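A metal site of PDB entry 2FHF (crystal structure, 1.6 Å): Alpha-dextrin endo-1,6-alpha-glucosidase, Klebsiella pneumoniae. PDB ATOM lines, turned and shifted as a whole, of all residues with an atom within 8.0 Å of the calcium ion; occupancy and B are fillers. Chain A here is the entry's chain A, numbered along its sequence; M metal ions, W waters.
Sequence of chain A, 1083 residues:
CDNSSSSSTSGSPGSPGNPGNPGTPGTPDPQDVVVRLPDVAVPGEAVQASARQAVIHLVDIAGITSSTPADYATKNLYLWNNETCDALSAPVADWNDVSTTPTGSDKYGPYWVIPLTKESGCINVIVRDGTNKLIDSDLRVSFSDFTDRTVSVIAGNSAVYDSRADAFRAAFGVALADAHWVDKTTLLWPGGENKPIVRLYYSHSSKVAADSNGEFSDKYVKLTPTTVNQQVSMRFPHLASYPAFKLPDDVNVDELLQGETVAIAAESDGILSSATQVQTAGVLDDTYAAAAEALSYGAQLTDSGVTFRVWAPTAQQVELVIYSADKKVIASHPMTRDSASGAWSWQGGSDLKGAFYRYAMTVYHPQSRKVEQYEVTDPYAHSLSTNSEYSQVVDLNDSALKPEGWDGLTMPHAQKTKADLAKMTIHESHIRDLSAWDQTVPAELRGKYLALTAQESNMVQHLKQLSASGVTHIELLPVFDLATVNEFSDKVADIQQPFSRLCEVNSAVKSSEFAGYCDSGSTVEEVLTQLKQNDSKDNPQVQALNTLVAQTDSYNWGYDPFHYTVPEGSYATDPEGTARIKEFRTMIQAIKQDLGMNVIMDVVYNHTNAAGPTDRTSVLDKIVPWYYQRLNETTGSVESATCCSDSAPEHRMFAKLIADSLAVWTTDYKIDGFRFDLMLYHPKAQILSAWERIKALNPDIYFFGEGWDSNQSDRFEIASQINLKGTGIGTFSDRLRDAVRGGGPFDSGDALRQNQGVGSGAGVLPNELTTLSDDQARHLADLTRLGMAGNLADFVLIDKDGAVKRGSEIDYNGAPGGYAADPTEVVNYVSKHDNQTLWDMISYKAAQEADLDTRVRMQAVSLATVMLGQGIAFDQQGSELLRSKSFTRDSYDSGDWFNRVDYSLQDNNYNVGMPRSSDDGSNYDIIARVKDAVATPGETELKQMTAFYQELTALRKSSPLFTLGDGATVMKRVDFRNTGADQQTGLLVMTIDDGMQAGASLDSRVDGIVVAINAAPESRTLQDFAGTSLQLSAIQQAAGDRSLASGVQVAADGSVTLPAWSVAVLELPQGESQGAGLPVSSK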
ATOM      1  N   LEU A 384     -35.146 -32.232 -17.210  1.00  0.00           N
ATOM      2  CA  LEU A 384     -33.791 -32.752 -17.248  1.00  0.00           C
ATOM      3  C   LEU A 384     -33.495 -33.695 -16.085  1.00  0.00           C
ATOM      4  O   LEU A 384     -34.221 -33.721 -15.101  1.00  0.00           O
ATOM      5  CB  LEU A 384     -32.790 -31.598 -17.157  1.00  0.00           C
ATOM      6  CG  LEU A 384     -32.779 -30.528 -18.261  1.00  0.00           C
ATOM      7  CD1 LEU A 384     -32.056 -29.276 -17.766  1.00  0.00           C
ATOM      8  CD2 LEU A 384     -32.074 -31.100 -19.498  1.00  0.00           C
ATOM      9  N   SER A 385     -32.413 -34.449 -16.232  1.00  0.00           N
ATOM     10  CA  SER A 385     -31.952 -35.346 -15.175  1.00  0.00           C
ATOM     11  C   SER A 385     -31.022 -34.475 -14.338  1.00  0.00           C
ATOM     12  O   SER A 385     -30.812 -33.302 -14.646  1.00  0.00           O
ATOM     13  CB  SER A 385     -31.166 -36.513 -15.766  1.00  0.00           C
ATOM     14  OG  SER A 385     -29.983 -36.060 -16.413  1.00  0.00           O
ATOM     15  N   THR A 386     -30.454 -35.040 -13.276  1.00  0.00           N
ATOM     16  CA  THR A 386     -29.547 -34.282 -12.415  1.00  0.00           C
ATOM     17  C   THR A 386     -28.346 -33.712 -13.174  1.00  0.00           C
ATOM     18  O   THR A 386     -27.657 -34.415 -13.918  1.00  0.00           O
ATOM     19  CB  THR A 386     -29.005 -35.166 -11.265  1.00  0.00           C
ATOM     20  OG1 THR A 386     -30.113 -35.660 -10.490  1.00  0.00           O
ATOM     21  CG2 THR A 386     -28.078 -34.358 -10.358  1.00  0.00           C
ATOM     22  N   ASN A 387     -28.100 -32.420 -12.970  1.00  0.00           N
ATOM     23  CA  ASN A 387     -27.001 -31.689 -13.595  1.00  0.00           C
ATOM     24  C   ASN A 387     -27.128 -31.570 -15.110  1.00  0.00           C
ATOM     25  O   ASN A 387     -26.131 -31.359 -15.809  1.00  0.00           O
ATOM     26  CB  ASN A 387     -25.646 -32.334 -13.233  1.00  0.00           C
ATOM     27  CG  ASN A 387     -24.529 -31.298 -13.092  1.00  0.00           C
ATOM     28  OD1 ASN A 387     -23.364 -31.574 -13.423  1.00  0.00           O
ATOM     29  ND2 ASN A 387     -24.858 -30.118 -12.581  1.00  0.00           N
ATOM     30  N   SER A 388     -28.347 -31.706 -15.616  1.00  0.00           N
ATOM     31  CA  SER A 388     -28.628 -31.552 -17.047  1.00  0.00           C
ATOM     32  C   SER A 388     -27.950 -32.532 -18.000  1.00  0.00           C
ATOM     33  O   SER A 388     -27.778 -32.211 -19.170  1.00  0.00           O
ATOM     34  CB  SER A 388     -28.257 -30.119 -17.478  1.00  0.00           C
ATOM     35  OG  SER A 388     -28.625 -29.163 -16.489  1.00  0.00           O
ATOM     36  N   PHE A 480     -33.698 -20.350 -14.497  1.00  0.00           N
ATOM     37  CA  PHE A 480     -33.775 -21.269 -15.618  1.00  0.00           C
ATOM     38  C   PHE A 480     -32.526 -22.119 -15.342  1.00  0.00           C
ATOM     39  O   PHE A 480     -31.800 -21.834 -14.385  1.00  0.00           O
ATOM     40  CB  PHE A 480     -33.646 -20.538 -16.960  1.00  0.00           C
ATOM     41  CG  PHE A 480     -32.506 -19.554 -16.995  1.00  0.00           C
ATOM     42  CD1 PHE A 480     -31.192 -19.979 -17.231  1.00  0.00           C
ATOM     43  CD2 PHE A 480     -32.731 -18.204 -16.751  1.00  0.00           C
ATOM     44  CE1 PHE A 480     -30.132 -19.070 -17.215  1.00  0.00           C
ATOM     45  CE2 PHE A 480     -31.686 -17.286 -16.733  1.00  0.00           C
ATOM     46  CZ  PHE A 480     -30.387 -17.725 -16.959  1.00  0.00           C
ATOM     47  N   ASP A 481     -32.253 -23.147 -16.146  1.00  0.00           N
ATOM     48  CA  ASP A 481     -31.101 -24.013 -15.882  1.00  0.00           C
ATOM     49  C   ASP A 481     -29.725 -23.399 -16.117  1.00  0.00           C
ATOM     50  O   ASP A 481     -29.293 -23.278 -17.270  1.00  0.00           O
ATOM     51  CB  ASP A 481     -31.219 -25.311 -16.676  1.00  0.00           C
ATOM     52  CG  ASP A 481     -30.084 -26.288 -16.395  1.00  0.00           C
ATOM     53  OD1 ASP A 481     -29.650 -26.373 -15.226  1.00  0.00           O
ATOM     54  OD2 ASP A 481     -29.632 -26.969 -17.332  1.00  0.00           O
ATOM     55  N   LEU A 482     -29.046 -23.029 -15.036  1.00  0.00           N
ATOM     56  CA  LEU A 482     -27.697 -22.473 -15.112  1.00  0.00           C
ATOM     57  C   LEU A 482     -26.690 -23.624 -15.064  1.00  0.00           C
ATOM     58  O   LEU A 482     -27.035 -24.735 -14.654  1.00  0.00           O
ATOM     59  CB  LEU A 482     -27.465 -21.489 -13.949  1.00  0.00           C
ATOM     60  CG  LEU A 482     -27.761 -21.965 -12.533  1.00  0.00           C
ATOM     61  CD1 LEU A 482     -26.476 -22.043 -11.729  1.00  0.00           C
ATOM     62  CD2 LEU A 482     -28.743 -20.984 -11.866  1.00  0.00           C
ATOM     63  N   ALA A 483     -25.451 -23.362 -15.466  1.00  0.00           N
ATOM     64  CA  ALA A 483     -24.431 -24.398 -15.524  1.00  0.00           C
ATOM     65  C   ALA A 483     -23.384 -24.373 -14.430  1.00  0.00           C
ATOM     66  O   ALA A 483     -22.750 -25.391 -14.170  1.00  0.00           O
ATOM     67  CB  ALA A 483     -23.732 -24.331 -16.877  1.00  0.00           C
ATOM     68  N   THR A 484     -23.248 -23.231 -13.778  1.00  0.00           N
ATOM     69  CA  THR A 484     -22.202 -23.023 -12.778  1.00  0.00           C
ATOM     70  C   THR A 484     -22.355 -23.532 -11.343  1.00  0.00           C
ATOM     71  O   THR A 484     -21.632 -23.095 -10.446  1.00  0.00           O
ATOM     72  CB  THR A 484     -21.826 -21.540 -12.765  1.00  0.00           C
ATOM     73  OG1 THR A 484     -23.019 -20.753 -12.729  1.00  0.00           O
ATOM     74  CG2 THR A 484     -21.039 -21.198 -14.028  1.00  0.00           C
ATOM     75  N   VAL A 485     -23.298 -24.445 -11.128  1.00  0.00           N
ATOM     76  CA  VAL A 485     -23.493 -25.075  -9.830  1.00  0.00           C
ATOM     77  C   VAL A 485     -23.690 -26.558 -10.115  1.00  0.00           C
ATOM     78  O   VAL A 485     -24.531 -26.933 -10.939  1.00  0.00           O
ATOM     79  CB  VAL A 485     -24.734 -24.528  -9.085  1.00  0.00           C
ATOM     80  CG1 VAL A 485     -25.065 -25.411  -7.896  1.00  0.00           C
ATOM     81  CG2 VAL A 485     -24.456 -23.104  -8.603  1.00  0.00           C
ATOM     82  N   ASN A 486     -22.901 -27.409  -9.473  1.00  0.00           N
ATOM     83  CA  ASN A 486     -23.043 -28.840  -9.701  1.00  0.00           C
ATOM     84  C   ASN A 486     -24.305 -29.303  -8.975  1.00  0.00           C
ATOM     85  O   ASN A 486     -24.442 -29.108  -7.768  1.00  0.00           O
ATOM     86  CB  ASN A 486     -21.819 -29.604  -9.187  1.00  0.00           C
ATOM     87  CG  ASN A 486     -21.734 -31.002  -9.747  1.00  0.00           C
ATOM     88  OD1 ASN A 486     -22.743 -31.700  -9.830  1.00  0.00           O
ATOM     89  ND2 ASN A 486     -20.539 -31.427 -10.134  1.00  0.00           N
ATOM     90  N   GLU A 487     -25.226 -29.919  -9.714  1.00  0.00           N
ATOM     91  CA  GLU A 487     -26.466 -30.381  -9.127  1.00  0.00           C
ATOM     92  C   GLU A 487     -26.361 -31.727  -8.405  1.00  0.00           C
ATOM     93  O   GLU A 487     -27.334 -32.173  -7.788  1.00  0.00           O
ATOM     94  CB  GLU A 487     -27.565 -30.415 -10.206  1.00  0.00           C
ATOM     95  CG  GLU A 487     -27.712 -29.085 -10.922  1.00  0.00           C
ATOM     96  CD  GLU A 487     -28.915 -28.999 -11.835  1.00  0.00           C
ATOM     97  OE1 GLU A 487     -29.511 -30.056 -12.171  1.00  0.00           O
ATOM     98  OE2 GLU A 487     -29.271 -27.865 -12.228  1.00  0.00           O
ATOM     99  N   ASP A 560     -25.352 -17.979 -16.577  1.00  0.00           N
ATOM    100  CA  ASP A 560     -24.614 -18.984 -17.347  1.00  0.00           C
ATOM    101  C   ASP A 560     -25.597 -20.037 -17.858  1.00  0.00           C
ATOM    102  O   ASP A 560     -25.664 -21.146 -17.326  1.00  0.00           O
ATOM    103  CB  ASP A 560     -23.590 -19.642 -16.427  1.00  0.00           C
ATOM    104  CG  ASP A 560     -22.762 -18.629 -15.646  1.00  0.00           C
ATOM    105  OD1 ASP A 560     -22.895 -18.559 -14.402  1.00  0.00           O
ATOM    106  OD2 ASP A 560     -21.982 -17.900 -16.293  1.00  0.00           O
ATOM    107  N   PRO A 561     -26.336 -19.709 -18.916  1.00  0.00           N
ATOM    108  CA  PRO A 561     -27.347 -20.576 -19.538  1.00  0.00           C
ATOM    109  C   PRO A 561     -26.899 -21.932 -20.053  1.00  0.00           C
ATOM    110  O   PRO A 561     -26.030 -22.021 -20.918  1.00  0.00           O
ATOM    111  CB  PRO A 561     -27.905 -19.710 -20.665  1.00  0.00           C
ATOM    112  CG  PRO A 561     -27.592 -18.302 -20.228  1.00  0.00           C
ATOM    113  CD  PRO A 561     -26.201 -18.461 -19.690  1.00  0.00           C
ATOM    114  N   PHE A 562     -27.512 -22.991 -19.511  1.00  0.00           N
ATOM    115  CA  PHE A 562     -27.232 -24.360 -19.926  1.00  0.00           C
ATOM    116  C   PHE A 562     -28.453 -24.764 -20.778  1.00  0.00           C
ATOM    117  O   PHE A 562     -28.301 -25.207 -21.916  1.00  0.00           O
ATOM    118  CB  PHE A 562     -27.080 -25.272 -18.701  1.00  0.00           C
ATOM    119  CG  PHE A 562     -26.377 -26.580 -18.972  1.00  0.00           C
ATOM    120  CD1 PHE A 562     -25.943 -27.373 -17.923  1.00  0.00           C
ATOM    121  CD2 PHE A 562     -26.150 -27.019 -20.280  1.00  0.00           C
ATOM    122  CE1 PHE A 562     -25.294 -28.582 -18.155  1.00  0.00           C
ATOM    123  CE2 PHE A 562     -25.498 -28.235 -20.528  1.00  0.00           C
ATOM    124  CZ  PHE A 562     -25.075 -29.014 -19.454  1.00  0.00           C
ATOM    125  N   HIS A 563     -29.652 -24.589 -20.213  1.00  0.00           N
ATOM    126  CA  HIS A 563     -30.927 -24.863 -20.913  1.00  0.00           C
ATOM    127  C   HIS A 563     -31.867 -23.703 -20.604  1.00  0.00           C
ATOM    128  O   HIS A 563     -32.120 -23.403 -19.436  1.00  0.00           O
ATOM    129  CB  HIS A 563     -31.522 -26.193 -20.442  1.00  0.00           C
ATOM    130  CG  HIS A 563     -30.678 -27.378 -20.767  1.00  0.00           C
ATOM    131  ND1 HIS A 563     -30.691 -27.987 -21.999  1.00  0.00           N
ATOM    132  CD2 HIS A 563     -29.705 -27.991 -20.060  1.00  0.00           C
ATOM    133  CE1 HIS A 563     -29.766 -28.924 -22.036  1.00  0.00           C
ATOM    134  NE2 HIS A 563     -29.144 -28.949 -20.869  1.00  0.00           N
ATOM    135  N   VAL A 566     -35.991 -24.813 -18.812  1.00  0.00           N
ATOM    136  CA  VAL A 566     -36.144 -25.808 -17.758  1.00  0.00           C
ATOM    137  C   VAL A 566     -35.708 -25.099 -16.480  1.00  0.00           C
ATOM    138  O   VAL A 566     -34.750 -24.329 -16.484  1.00  0.00           O
ATOM    139  CB  VAL A 566     -35.215 -27.018 -17.934  1.00  0.00           C
ATOM    140  CG1 VAL A 566     -35.588 -28.088 -16.907  1.00  0.00           C
ATOM    141  CG2 VAL A 566     -35.297 -27.570 -19.348  1.00  0.00           C
ATOM    142  N   PRO A 567     -36.421 -25.330 -15.362  1.00  0.00           N
ATOM    143  CA  PRO A 567     -36.021 -24.667 -14.117  1.00  0.00           C
ATOM    144  C   PRO A 567     -34.662 -25.204 -13.656  1.00  0.00           C
ATOM    145  O   PRO A 567     -34.292 -26.327 -13.991  1.00  0.00           O
ATOM    146  CB  PRO A 567     -37.136 -25.062 -13.143  1.00  0.00           C
ATOM    147  CG  PRO A 567     -38.330 -25.158 -14.034  1.00  0.00           C
ATOM    148  CD  PRO A 567     -37.789 -25.889 -15.244  1.00  0.00           C
ATOM    149  N   GLU A 568     -33.927 -24.394 -12.891  1.00  0.00           N
ATOM    150  CA  GLU A 568     -32.628 -24.792 -12.351  1.00  0.00           C
ATOM    151  C   GLU A 568     -32.839 -25.968 -11.378  1.00  0.00           C
ATOM    152  O   GLU A 568     -33.793 -25.966 -10.605  1.00  0.00           O
ATOM    153  CB  GLU A 568     -31.982 -23.611 -11.633  1.00  0.00           C
ATOM    154  CG  GLU A 568     -30.892 -23.994 -10.633  1.00  0.00           C
ATOM    155  CD  GLU A 568     -29.711 -24.711 -11.241  1.00  0.00           C
ATOM    156  OE1 GLU A 568     -28.859 -25.206 -10.474  1.00  0.00           O
ATOM    157  OE2 GLU A 568     -29.606 -24.792 -12.491  1.00  0.00           O
ATOM    158  N   GLY A 569     -31.941 -26.939 -11.413  1.00  0.00           N
ATOM    159  CA  GLY A 569     -32.078 -28.101 -10.539  1.00  0.00           C
ATOM    160  C   GLY A 569     -31.613 -27.998  -9.105  1.00  0.00           C
ATOM    161  O   GLY A 569     -32.230 -28.584  -8.209  1.00  0.00           O
ATOM    162  N   SER A 570     -30.539 -27.259  -8.856  1.00  0.00           N
ATOM    163  CA  SER A 570     -30.019 -27.131  -7.491  1.00  0.00           C
ATOM    164  C   SER A 570     -30.967 -26.408  -6.535  1.00  0.00           C
ATOM    165  O   SER A 570     -30.815 -26.523  -5.319  1.00  0.00           O
ATOM    166  CB  SER A 570     -28.651 -26.412  -7.510  1.00  0.00           C
ATOM    167  OG  SER A 570     -28.793 -25.047  -7.838  1.00  0.00           O
ATOM    168  N   TYR A 571     -31.945 -25.679  -7.067  1.00  0.00           N
ATOM    169  CA  TYR A 571     -32.902 -24.979  -6.214  1.00  0.00           C
ATOM    170  C   TYR A 571     -34.117 -25.861  -5.867  1.00  0.00           C
ATOM    171  O   TYR A 571     -35.033 -25.426  -5.171  1.00  0.00           O
ATOM    172  CB  TYR A 571     -33.381 -23.674  -6.879  1.00  0.00           C
ATOM    173  CG  TYR A 571     -32.287 -22.649  -7.107  1.00  0.00           C
ATOM    174  CD1 TYR A 571     -31.259 -22.484  -6.180  1.00  0.00           C
ATOM    175  CD2 TYR A 571     -32.294 -21.826  -8.233  1.00  0.00           C
ATOM    176  CE1 TYR A 571     -30.264 -21.520  -6.375  1.00  0.00           C
ATOM    177  CE2 TYR A 571     -31.306 -20.860  -8.436  1.00  0.00           C
ATOM    178  CZ  TYR A 571     -30.291 -20.719  -7.503  1.00  0.00           C
ATOM    179  OH  TYR A 571     -29.301 -19.786  -7.700  1.00  0.00           O
ATOM    180  N   PRO A 575     -33.318 -32.797  -7.716  1.00  0.00           N
ATOM    181  CA  PRO A 575     -32.952 -32.394  -9.074  1.00  0.00           C
ATOM    182  C   PRO A 575     -33.067 -33.464 -10.154  1.00  0.00           C
ATOM    183  O   PRO A 575     -32.763 -33.216 -11.319  1.00  0.00           O
ATOM    184  CB  PRO A 575     -31.510 -31.932  -8.902  1.00  0.00           C
ATOM    185  CG  PRO A 575     -31.000 -32.941  -7.911  1.00  0.00           C
ATOM    186  CD  PRO A 575     -32.119 -33.004  -6.891  1.00  0.00           C
ATOM    187  N   ARG A 580     -38.625 -30.882  -9.941  1.00  0.00           N
ATOM    188  CA  ARG A 580     -38.359 -29.446  -9.870  1.00  0.00           C
ATOM    189  C   ARG A 580     -39.464 -28.588 -10.494  1.00  0.00           C
ATOM    190  O   ARG A 580     -39.649 -27.430 -10.110  1.00  0.00           O
ATOM    191  CB  ARG A 580     -37.023 -29.128 -10.543  1.00  0.00           C
ATOM    192  CG  ARG A 580     -37.077 -29.158 -12.059  1.00  0.00           C
ATOM    193  CD  ARG A 580     -35.710 -28.842 -12.678  1.00  0.00           C
ATOM    194  NE  ARG A 580     -34.775 -29.963 -12.577  1.00  0.00           N
ATOM    195  CZ  ARG A 580     -33.624 -30.025 -13.223  1.00  0.00           C
ATOM    196  NH1 ARG A 580     -33.244 -29.020 -14.017  1.00  0.00           N
ATOM    197  NH2 ARG A 580     -32.836 -31.093 -13.104  1.00  0.00           N
ATOM    198  N   ARG A 616     -18.750 -29.547 -22.049  1.00  0.00           N
ATOM    199  CA  ARG A 616     -19.914 -30.239 -21.508  1.00  0.00           C
ATOM    200  C   ARG A 616     -21.206 -29.429 -21.623  1.00  0.00           C
ATOM    201  O   ARG A 616     -22.276 -29.989 -21.878  1.00  0.00           O
ATOM    202  CB  ARG A 616     -19.664 -30.546 -20.029  1.00  0.00           C
ATOM    203  CG  ARG A 616     -20.898 -30.991 -19.244  1.00  0.00           C
ATOM    204  CD  ARG A 616     -20.586 -31.156 -17.762  1.00  0.00           C
ATOM    205  NE  ARG A 616     -20.261 -29.899 -17.088  1.00  0.00           N
ATOM    206  CZ  ARG A 616     -21.128 -29.158 -16.422  1.00  0.00           C
ATOM    207  NH1 ARG A 616     -22.394 -29.531 -16.299  1.00  0.00           N
ATOM    208  NH2 ARG A 616     -20.728 -28.024 -15.837  1.00  0.00           N
HETATM  209 CA    CA M   1     -28.263 -26.348 -13.583  1.00  0.00          CA
HETATM  210  O   HOH W   1     -26.764 -25.872 -11.982  1.00  0.00           O
HETATM  211  O   HOH W   2     -26.983 -27.990 -14.507  1.00  0.00           O
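OG of Ser 388 is in hydrogen-bond range of OD2 of Asp 481, at 2.6 Å. The backbone carbonyl oxygen of Asp 481 is in hydrogen-bond range of the backbone NH of Phe 562, 2.9 Å away. The backbone carbonyl oxygen (O) of Asp 481 lies within hydrogen-bond range of the backbone NH (N) of His 563, 3.2 Å away. O of Val 566 is in hydrogen-bond range of N of Asp 481 (2.8 Å). The side-chain carboxylate (OE2) of Glu 487 lies close to the backbone NH (N) of Gly 569 (2.9 Å). N of Asn 387 lies within hydrogen-bond range of OE1 of Glu 487, at 2.9 Å. OE1 of Glu 487 lies within salt-bridge range of NH2 of Arg 580 (3.6 Å). The side-chain carboxylate of Glu 568 is in hydrogen-bond range of the side-chain hydroxyl of Ser 570.
Four residues have an atom within 4 Å of the calcium ion: Asp 481, Leu 482, Glu 487 and Glu 568.
The calcium ion is bound by OD1 of Asp 481. Water W1 is bound to the calcium ion, 2.2 Å away. OE2 of Glu 487 is bound to the calcium ion (2.3 Å). Water W2 is bound to the calcium ion (2.3 Å). O of Leu 482 binds the calcium ion (2.3 Å). OE2 of Glu 568 is bound to the calcium ion, 2.3 Å away.
Water W1 bridges the side-chain carboxylate of Glu 568 (2.7 Å) and the backbone carbonyl oxygen of Val 485 (2.7 Å).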
